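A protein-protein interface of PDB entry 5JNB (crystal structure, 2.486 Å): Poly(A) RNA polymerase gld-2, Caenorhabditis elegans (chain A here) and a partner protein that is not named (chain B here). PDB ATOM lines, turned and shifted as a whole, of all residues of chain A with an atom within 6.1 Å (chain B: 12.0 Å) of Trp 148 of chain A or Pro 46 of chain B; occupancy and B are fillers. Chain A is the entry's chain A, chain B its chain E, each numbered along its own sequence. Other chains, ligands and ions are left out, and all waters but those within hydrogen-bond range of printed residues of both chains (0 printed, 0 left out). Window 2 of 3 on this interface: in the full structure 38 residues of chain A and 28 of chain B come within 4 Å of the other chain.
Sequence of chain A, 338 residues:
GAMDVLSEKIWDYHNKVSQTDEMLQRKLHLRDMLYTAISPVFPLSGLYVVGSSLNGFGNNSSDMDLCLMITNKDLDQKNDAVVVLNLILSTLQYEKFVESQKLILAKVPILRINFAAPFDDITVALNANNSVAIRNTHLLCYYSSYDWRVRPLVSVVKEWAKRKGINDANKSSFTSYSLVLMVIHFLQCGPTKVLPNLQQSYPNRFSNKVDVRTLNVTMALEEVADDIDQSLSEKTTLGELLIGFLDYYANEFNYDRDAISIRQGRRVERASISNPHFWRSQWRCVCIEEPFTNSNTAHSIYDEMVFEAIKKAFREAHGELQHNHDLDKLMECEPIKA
NH1 of Arg 151 of chain A lies within hydrogen-bond range of OG1 of Thr 42 of chain B (3.0 Å).
The side-chain hydroxyl (OG) of Ser 145 of chain A lies within hydrogen-bond range of the side-chain hydroxyl (OG) of Ser 41 of chain B, at 3.4 Å.
The side-chain hydroxyl (OG) of Ser 145 of chain A is in hydrogen-bond range of the backbone carbonyl oxygen (O) of Leu 37 of chain B, 3.5 Å away.
The backbone carbonyl oxygen of Ile 38 of chain B lies within hydrogen-bond range of the side-chain hydroxyl of Ser 41 of chain B (2.9 Å).
OG1 of Thr 42 of chain B is in hydrogen-bond range of O of Ile 38 of chain B (3.0 Å).
NE1 of Trp 148 of chain A lies within hydrogen-bond range of OE1 of Glu 234 of chain A (3.1 Å).
The side-chain hydroxyl (OG) of Ser 41 of chain B sits at hydrogen-bond distance from the backbone carbonyl oxygen (O) of Leu 37 of chain B (2.9 Å).
The backbone carbonyl oxygen (O) of Leu 37 of chain B sits at hydrogen-bond distance from the side-chain hydroxyl (OG) of Ser 40 of chain B (3.5 Å).
Trp 11 of chain A touches Pro 43 of chain B (CH2 to O, 3.9 Å).
CZ2 of Trp 11 of chain A touches CD of Pro 46 of chain B, 3.5 Å away.
Trp 148 of chain A touches Pro 43 of chain B.
Pro 46 of chain B touches Trp 148 of chain A.
Arg 151 of chain A touches Ile 38 of chain B (CZ to CG2, 3.7 Å).
Trp 11 of chain A touches two residues of chain B.
Ser 144 of chain A touches none of the printed residues of chain B.
Printed residues of chain B within 4 Å of Ser 145 of chain A: Leu 37 (3.5 Å) and Ser 41 (3.4 Å).
Asp 147 of chain A touches none of the printed residues of chain B.
Trp 148 of chain A touches just these residues of chain B: Pro 43 (3.8 Å) and Pro 46 (3.6 Å).
Arg 149 of chain A touches none of the printed residues of chain B.
Val 150 of chain A touches none of the printed residues of chain B.
Pro 152 of chain A touches none of the printed residues of chain B.
Of the printed residues of chain A, Leu 37 of chain B touches Ser 145 (3.5 Å).
Pro 46 of chain B touches two residues of chain A.
The nearest residue of chain B that does not touch Trp 148 of chain A is Ser 41 of chain B (4.6 Å).
The nearest printed residue of chain A that does not touch Pro 46 of chain B is Leu 238 of chain A (7.3 Å).
The nearest printed residue of chain A that does not touch Pro 43 of chain B is Arg 151 of chain A (6.7 Å).
Of the 13 printed residues of chain A, 4 touch a printed residue of chain B.
Hydrophobic or aromatic side chains of chain A that line the printed part of chain B: Trp 11 and Trp 148.
Of the 10 printed residues of chain B, 6 touch a printed residue of chain A.
Printed residues of chain B that touch a printed residue of chain A: Leu 37, Ile 38, Ser 41, Thr 42, Pro 43 and Pro 46.
Hydrophobic or aromatic side chains of chain B within 4 Å of the printed part of chain A: Leu 37, Ile 38, Pro 43 and Pro 46.
Among the printed residues, 8 pairs touch across the chains.
Among the printed residues, no Asp or Glu carboxylate lies within 4 Å of a Lys or Arg side-chain nitrogen of the other chain.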
ATOM      1  N   TRP A  11      17.211  27.552   4.600  1.00  0.00           N
ATOM      2  CA  TRP A  11      17.808  26.233   4.700  1.00  0.00           C
ATOM      3  C   TRP A  11      19.226  26.199   4.138  1.00  0.00           C
ATOM      4  O   TRP A  11      20.124  25.612   4.723  1.00  0.00           O
ATOM      5  CB  TRP A  11      16.923  25.227   3.973  1.00  0.00           C
ATOM      6  CG  TRP A  11      17.510  23.881   3.889  1.00  0.00           C
ATOM      7  CD1 TRP A  11      18.152  23.339   2.823  1.00  0.00           C
ATOM      8  CD2 TRP A  11      17.530  22.886   4.922  1.00  0.00           C
ATOM      9  NE1 TRP A  11      18.566  22.065   3.118  1.00  0.00           N
ATOM     10  CE2 TRP A  11      18.200  21.764   4.403  1.00  0.00           C
ATOM     11  CE3 TRP A  11      17.047  22.837   6.233  1.00  0.00           C
ATOM     12  CZ2 TRP A  11      18.398  20.600   5.147  1.00  0.00           C
ATOM     13  CZ3 TRP A  11      17.246  21.674   6.971  1.00  0.00           C
ATOM     14  CH2 TRP A  11      17.916  20.575   6.422  1.00  0.00           C
ATOM     15  N   SER A 144      16.353  21.206  19.715  1.00  0.00           N
ATOM     16  CA  SER A 144      17.012  21.259  18.423  1.00  0.00           C
ATOM     17  C   SER A 144      16.632  20.107  17.478  1.00  0.00           C
ATOM     18  O   SER A 144      16.671  20.265  16.250  1.00  0.00           O
ATOM     19  CB  SER A 144      18.522  21.280  18.650  1.00  0.00           C
ATOM     20  OG  SER A 144      19.218  20.676  17.586  1.00  0.00           O
ATOM     21  N   SER A 145      16.267  18.960  18.056  1.00  0.00           N
ATOM     22  CA  SER A 145      16.057  17.728  17.298  1.00  0.00           C
ATOM     23  C   SER A 145      14.587  17.452  17.038  1.00  0.00           C
ATOM     24  O   SER A 145      14.244  16.669  16.157  1.00  0.00           O
ATOM     25  CB  SER A 145      16.660  16.526  18.036  1.00  0.00           C
ATOM     26  OG  SER A 145      18.070  16.601  18.077  1.00  0.00           O
ATOM     27  N   TYR A 146      13.729  18.084  17.826  1.00  0.00           N
ATOM     28  CA  TYR A 146      12.303  17.824  17.773  1.00  0.00           C
ATOM     29  C   TYR A 146      11.653  18.043  16.406  1.00  0.00           C
ATOM     30  O   TYR A 146      10.738  17.324  16.037  1.00  0.00           O
ATOM     31  CB  TYR A 146      11.597  18.692  18.796  1.00  0.00           C
ATOM     32  CG  TYR A 146      10.199  18.234  19.072  1.00  0.00           C
ATOM     33  CD1 TYR A 146       9.939  17.345  20.099  1.00  0.00           C
ATOM     34  CD2 TYR A 146       9.135  18.676  18.299  1.00  0.00           C
ATOM     35  CE1 TYR A 146       8.655  16.929  20.366  1.00  0.00           C
ATOM     36  CE2 TYR A 146       7.848  18.252  18.555  1.00  0.00           C
ATOM     37  CZ  TYR A 146       7.614  17.379  19.591  1.00  0.00           C
ATOM     38  OH  TYR A 146       6.337  16.953  19.859  1.00  0.00           O
ATOM     39  N   ASP A 147      12.123  19.044  15.669  1.00  0.00           N
ATOM     40  CA  ASP A 147      11.510  19.442  14.406  1.00  0.00           C
ATOM     41  C   ASP A 147      12.617  19.998  13.516  1.00  0.00           C
ATOM     42  O   ASP A 147      13.456  20.774  13.985  1.00  0.00           O
ATOM     43  CB  ASP A 147      10.402  20.470  14.672  1.00  0.00           C
ATOM     44  CG  ASP A 147       9.616  20.844  13.428  1.00  0.00           C
ATOM     45  OD1 ASP A 147      10.187  21.452  12.486  1.00  0.00           O
ATOM     46  OD2 ASP A 147       8.398  20.560  13.424  1.00  0.00           O
ATOM     47  N   TRP A 148      12.644  19.603  12.246  1.00  0.00           N
ATOM     48  CA  TRP A 148      13.761  19.971  11.370  1.00  0.00           C
ATOM     49  C   TRP A 148      13.875  21.476  11.130  1.00  0.00           C
ATOM     50  O   TRP A 148      14.930  21.952  10.755  1.00  0.00           O
ATOM     51  CB  TRP A 148      13.646  19.273  10.015  1.00  0.00           C
ATOM     52  CG  TRP A 148      12.584  19.872   9.153  1.00  0.00           C
ATOM     53  CD1 TRP A 148      11.227  19.702   9.278  1.00  0.00           C
ATOM     54  CD2 TRP A 148      12.777  20.752   8.041  1.00  0.00           C
ATOM     55  NE1 TRP A 148      10.569  20.431   8.313  1.00  0.00           N
ATOM     56  CE2 TRP A 148      11.498  21.075   7.536  1.00  0.00           C
ATOM     57  CE3 TRP A 148      13.906  21.289   7.415  1.00  0.00           C
ATOM     58  CZ2 TRP A 148      11.322  21.922   6.435  1.00  0.00           C
ATOM     59  CZ3 TRP A 148      13.728  22.134   6.326  1.00  0.00           C
ATOM     60  CH2 TRP A 148      12.447  22.443   5.849  1.00  0.00           C
ATOM     61  N   ARG A 149      12.796  22.223  11.324  1.00  0.00           N
ATOM     62  CA  ARG A 149      12.840  23.649  11.038  1.00  0.00           C
ATOM     63  C   ARG A 149      13.543  24.447  12.142  1.00  0.00           C
ATOM     64  O   ARG A 149      13.997  25.563  11.894  1.00  0.00           O
ATOM     65  CB  ARG A 149      11.423  24.203  10.828  1.00  0.00           C
ATOM     66  CG  ARG A 149      10.748  23.746   9.536  1.00  0.00           C
ATOM     67  CD  ARG A 149       9.245  23.966   9.598  1.00  0.00           C
ATOM     68  NE  ARG A 149       8.618  23.048  10.541  1.00  0.00           N
ATOM     69  CZ  ARG A 149       7.333  23.086  10.864  1.00  0.00           C
ATOM     70  NH1 ARG A 149       6.554  23.999  10.306  1.00  0.00           N
ATOM     71  NH2 ARG A 149       6.831  22.223  11.742  1.00  0.00           N
ATOM     72  N   VAL A 150      13.629  23.878  13.349  1.00  0.00           N
ATOM     73  CA  VAL A 150      14.154  24.600  14.512  1.00  0.00           C
ATOM     74  C   VAL A 150      15.590  25.112  14.308  1.00  0.00           C
ATOM     75  O   VAL A 150      15.850  26.310  14.464  1.00  0.00           O
ATOM     76  CB  VAL A 150      14.103  23.714  15.788  1.00  0.00           C
ATOM     77  CG1 VAL A 150      14.874  24.368  16.939  1.00  0.00           C
ATOM     78  CG2 VAL A 150      12.669  23.477  16.201  1.00  0.00           C
ATOM     79  N   ARG A 151      16.512  24.222  13.941  1.00  0.00           N
ATOM     80  CA  ARG A 151      17.918  24.616  13.792  1.00  0.00           C
ATOM     81  C   ARG A 151      18.194  25.648  12.676  1.00  0.00           C
ATOM     82  O   ARG A 151      18.966  26.589  12.883  1.00  0.00           O
ATOM     83  CB  ARG A 151      18.794  23.374  13.581  1.00  0.00           C
ATOM     84  CG  ARG A 151      18.880  22.493  14.811  1.00  0.00           C
ATOM     85  CD  ARG A 151      19.518  21.155  14.509  1.00  0.00           C
ATOM     86  NE  ARG A 151      20.904  21.353  14.129  1.00  0.00           N
ATOM     87  CZ  ARG A 151      21.505  20.730  13.124  1.00  0.00           C
ATOM     88  NH1 ARG A 151      20.833  19.848  12.389  1.00  0.00           N
ATOM     89  NH2 ARG A 151      22.780  21.000  12.851  1.00  0.00           N
ATOM     90  N   PRO A 152      17.601  25.471  11.485  1.00  0.00           N
ATOM     91  CA  PRO A 152      17.891  26.503  10.484  1.00  0.00           C
ATOM     92  C   PRO A 152      17.225  27.840  10.783  1.00  0.00           C
ATOM     93  O   PRO A 152      17.742  28.867  10.363  1.00  0.00           O
ATOM     94  CB  PRO A 152      17.346  25.898   9.185  1.00  0.00           C
ATOM     95  CG  PRO A 152      16.457  24.787   9.597  1.00  0.00           C
ATOM     96  CD  PRO A 152      16.980  24.278  10.883  1.00  0.00           C
ATOM     97  N   LEU A 153      16.103  27.839  11.489  1.00  0.00           N
ATOM     98  CA  LEU A 153      15.519  29.088  11.948  1.00  0.00           C
ATOM     99  C   LEU A 153      16.514  29.801  12.877  1.00  0.00           C
ATOM    100  O   LEU A 153      16.752  31.014  12.755  1.00  0.00           O
ATOM    101  CB  LEU A 153      14.191  28.829  12.652  1.00  0.00           C
ATOM    102  CG  LEU A 153      13.394  29.987  13.250  1.00  0.00           C
ATOM    103  CD1 LEU A 153      13.170  31.123  12.245  1.00  0.00           C
ATOM    104  CD2 LEU A 153      12.061  29.441  13.754  1.00  0.00           C
ATOM    105  N   GLU A 234       2.954  21.578  10.318  1.00  0.00           N
ATOM    106  CA  GLU A 234       3.761  21.444   9.109  1.00  0.00           C
ATOM    107  C   GLU A 234       3.157  22.209   7.935  1.00  0.00           C
ATOM    108  O   GLU A 234       3.782  22.349   6.888  1.00  0.00           O
ATOM    109  CB  GLU A 234       3.951  19.971   8.750  1.00  0.00           C
ATOM    110  CG  GLU A 234       5.329  19.659   8.157  1.00  0.00           C
ATOM    111  CD  GLU A 234       6.491  20.018   9.091  1.00  0.00           C
ATOM    112  OE1 GLU A 234       7.524  20.541   8.590  1.00  0.00           O
ATOM    113  OE2 GLU A 234       6.378  19.762  10.319  1.00  0.00           O
ATOM    114  N   LEU A 238       9.053  27.275   6.611  1.00  0.00           N
ATOM    115  CA  LEU A 238      10.193  27.825   7.314  1.00  0.00           C
ATOM    116  C   LEU A 238      10.188  29.347   7.184  1.00  0.00           C
ATOM    117  O   LEU A 238      10.185  30.065   8.189  1.00  0.00           O
ATOM    118  CB  LEU A 238      11.469  27.213   6.752  1.00  0.00           C
ATOM    119  CG  LEU A 238      12.817  27.397   7.417  1.00  0.00           C
ATOM    120  CD1 LEU A 238      12.724  27.190   8.925  1.00  0.00           C
ATOM    121  CD2 LEU A 238      13.742  26.375   6.777  1.00  0.00           C
ATOM    122  N   LEU B  37      22.113  12.086  17.889  1.00  0.00           N
ATOM    123  CA  LEU B  37      20.745  12.572  18.014  1.00  0.00           C
ATOM    124  C   LEU B  37      20.471  13.698  17.042  1.00  0.00           C
ATOM    125  O   LEU B  37      19.372  13.821  16.498  1.00  0.00           O
ATOM    126  CB  LEU B  37      20.472  13.062  19.436  1.00  0.00           C
ATOM    127  CG  LEU B  37      19.003  13.340  19.723  1.00  0.00           C
ATOM    128  CD1 LEU B  37      18.265  12.032  20.042  1.00  0.00           C
ATOM    129  CD2 LEU B  37      18.872  14.355  20.854  1.00  0.00           C
ATOM    130  N   ILE B  38      21.480  14.534  16.844  1.00  0.00           N
ATOM    131  CA  ILE B  38      21.350  15.678  15.967  1.00  0.00           C
ATOM    132  C   ILE B  38      21.324  15.190  14.529  1.00  0.00           C
ATOM    133  O   ILE B  38      20.441  15.545  13.754  1.00  0.00           O
ATOM    134  CB  ILE B  38      22.514  16.687  16.187  1.00  0.00           C
ATOM    135  CG1 ILE B  38      22.390  17.339  17.572  1.00  0.00           C
ATOM    136  CG2 ILE B  38      22.557  17.736  15.086  1.00  0.00           C
ATOM    137  CD1 ILE B  38      23.699  17.916  18.121  1.00  0.00           C
ATOM    138  N   ARG B  39      22.299  14.350  14.204  1.00  0.00           N
ATOM    139  CA  ARG B  39      22.521  13.872  12.848  1.00  0.00           C
ATOM    140  C   ARG B  39      21.389  12.963  12.390  1.00  0.00           C
ATOM    141  O   ARG B  39      21.015  12.966  11.216  1.00  0.00           O
ATOM    142  CB  ARG B  39      23.861  13.142  12.782  1.00  0.00           C
ATOM    143  CG  ARG B  39      24.573  13.216  11.451  1.00  0.00           C
ATOM    144  CD  ARG B  39      26.083  13.168  11.668  1.00  0.00           C
ATOM    145  NE  ARG B  39      26.432  12.260  12.760  1.00  0.00           N
ATOM    146  CZ  ARG B  39      27.389  12.482  13.659  1.00  0.00           C
ATOM    147  NH1 ARG B  39      28.121  13.594  13.602  1.00  0.00           N
ATOM    148  NH2 ARG B  39      27.621  11.587  14.616  1.00  0.00           N
ATOM    149  N   SER B  40      20.832  12.197  13.318  1.00  0.00           N
ATOM    150  CA  SER B  40      19.754  11.284  12.979  1.00  0.00           C
ATOM    151  C   SER B  40      18.405  11.997  12.857  1.00  0.00           C
ATOM    152  O   SER B  40      17.419  11.392  12.430  1.00  0.00           O
ATOM    153  CB  SER B  40      19.662  10.170  14.016  1.00  0.00           C
ATOM    154  OG  SER B  40      18.997  10.630  15.182  1.00  0.00           O
ATOM    155  N   SER B  41      18.352  13.273  13.228  1.00  0.00           N
ATOM    156  CA  SER B  41      17.114  14.042  13.092  1.00  0.00           C
ATOM    157  C   SER B  41      17.237  15.122  12.009  1.00  0.00           C
ATOM    158  O   SER B  41      16.347  15.953  11.829  1.00  0.00           O
ATOM    159  CB  SER B  41      16.721  14.670  14.424  1.00  0.00           C
ATOM    160  OG  SER B  41      17.719  15.561  14.873  1.00  0.00           O
ATOM    161  N   THR B  42      18.341  15.079  11.272  1.00  0.00           N
ATOM    162  CA  THR B  42      18.531  15.948  10.117  1.00  0.00           C
ATOM    163  C   THR B  42      18.177  15.252   8.799  1.00  0.00           C
ATOM    164  O   THR B  42      18.858  14.311   8.393  1.00  0.00           O
ATOM    165  CB  THR B  42      19.984  16.448  10.025  1.00  0.00           C
ATOM    166  OG1 THR B  42      20.318  17.156  11.224  1.00  0.00           O
ATOM    167  CG2 THR B  42      20.152  17.371   8.828  1.00  0.00           C
ATOM    168  N   PRO B  43      17.116  15.727   8.125  1.00  0.00           N
ATOM    169  CA  PRO B  43      16.704  15.238   6.801  1.00  0.00           C
ATOM    170  C   PRO B  43      17.741  15.583   5.739  1.00  0.00           C
ATOM    171  O   PRO B  43      18.269  16.697   5.783  1.00  0.00           O
ATOM    172  CB  PRO B  43      15.395  15.982   6.541  1.00  0.00           C
ATOM    173  CG  PRO B  43      15.534  17.251   7.338  1.00  0.00           C
ATOM    174  CD  PRO B  43      16.264  16.839   8.588  1.00  0.00           C
ATOM    175  N   THR B  44      18.010  14.658   4.813  1.00  0.00           N
ATOM    176  CA  THR B  44      19.132  14.792   3.877  1.00  0.00           C
ATOM    177  C   THR B  44      18.828  15.771   2.743  1.00  0.00           C
ATOM    178  O   THR B  44      19.740  16.375   2.170  1.00  0.00           O
ATOM    179  CB  THR B  44      19.541  13.421   3.262  1.00  0.00           C
ATOM    180  OG1 THR B  44      18.573  13.018   2.289  1.00  0.00           O
ATOM    181  CG2 THR B  44      19.649  12.342   4.332  1.00  0.00           C
ATOM    182  N   ASP B  45      17.547  15.929   2.427  1.00  0.00           N
ATOM    183  CA  ASP B  45      17.120  16.883   1.406  1.00  0.00           C
ATOM    184  C   ASP B  45      15.613  17.110   1.467  1.00  0.00           C
ATOM    185  O   ASP B  45      14.860  16.415   0.793  1.00  0.00           O
ATOM    186  CB  ASP B  45      17.518  16.398   0.007  1.00  0.00           C
ATOM    187  N   PRO B  46      15.171  18.084   2.281  1.00  0.00           N
ATOM    188  CA  PRO B  46      13.746  18.388   2.450  1.00  0.00           C
ATOM    189  C   PRO B  46      13.181  19.214   1.297  1.00  0.00           C
ATOM    190  O   PRO B  46      12.030  19.641   1.395  1.00  0.00           O
ATOM    191  CB  PRO B  46      13.719  19.188   3.753  1.00  0.00           C
ATOM    192  CG  PRO B  46      15.027  19.907   3.754  1.00  0.00           C
ATOM    193  CD  PRO B  46      16.018  18.943   3.131  1.00  0.00           C
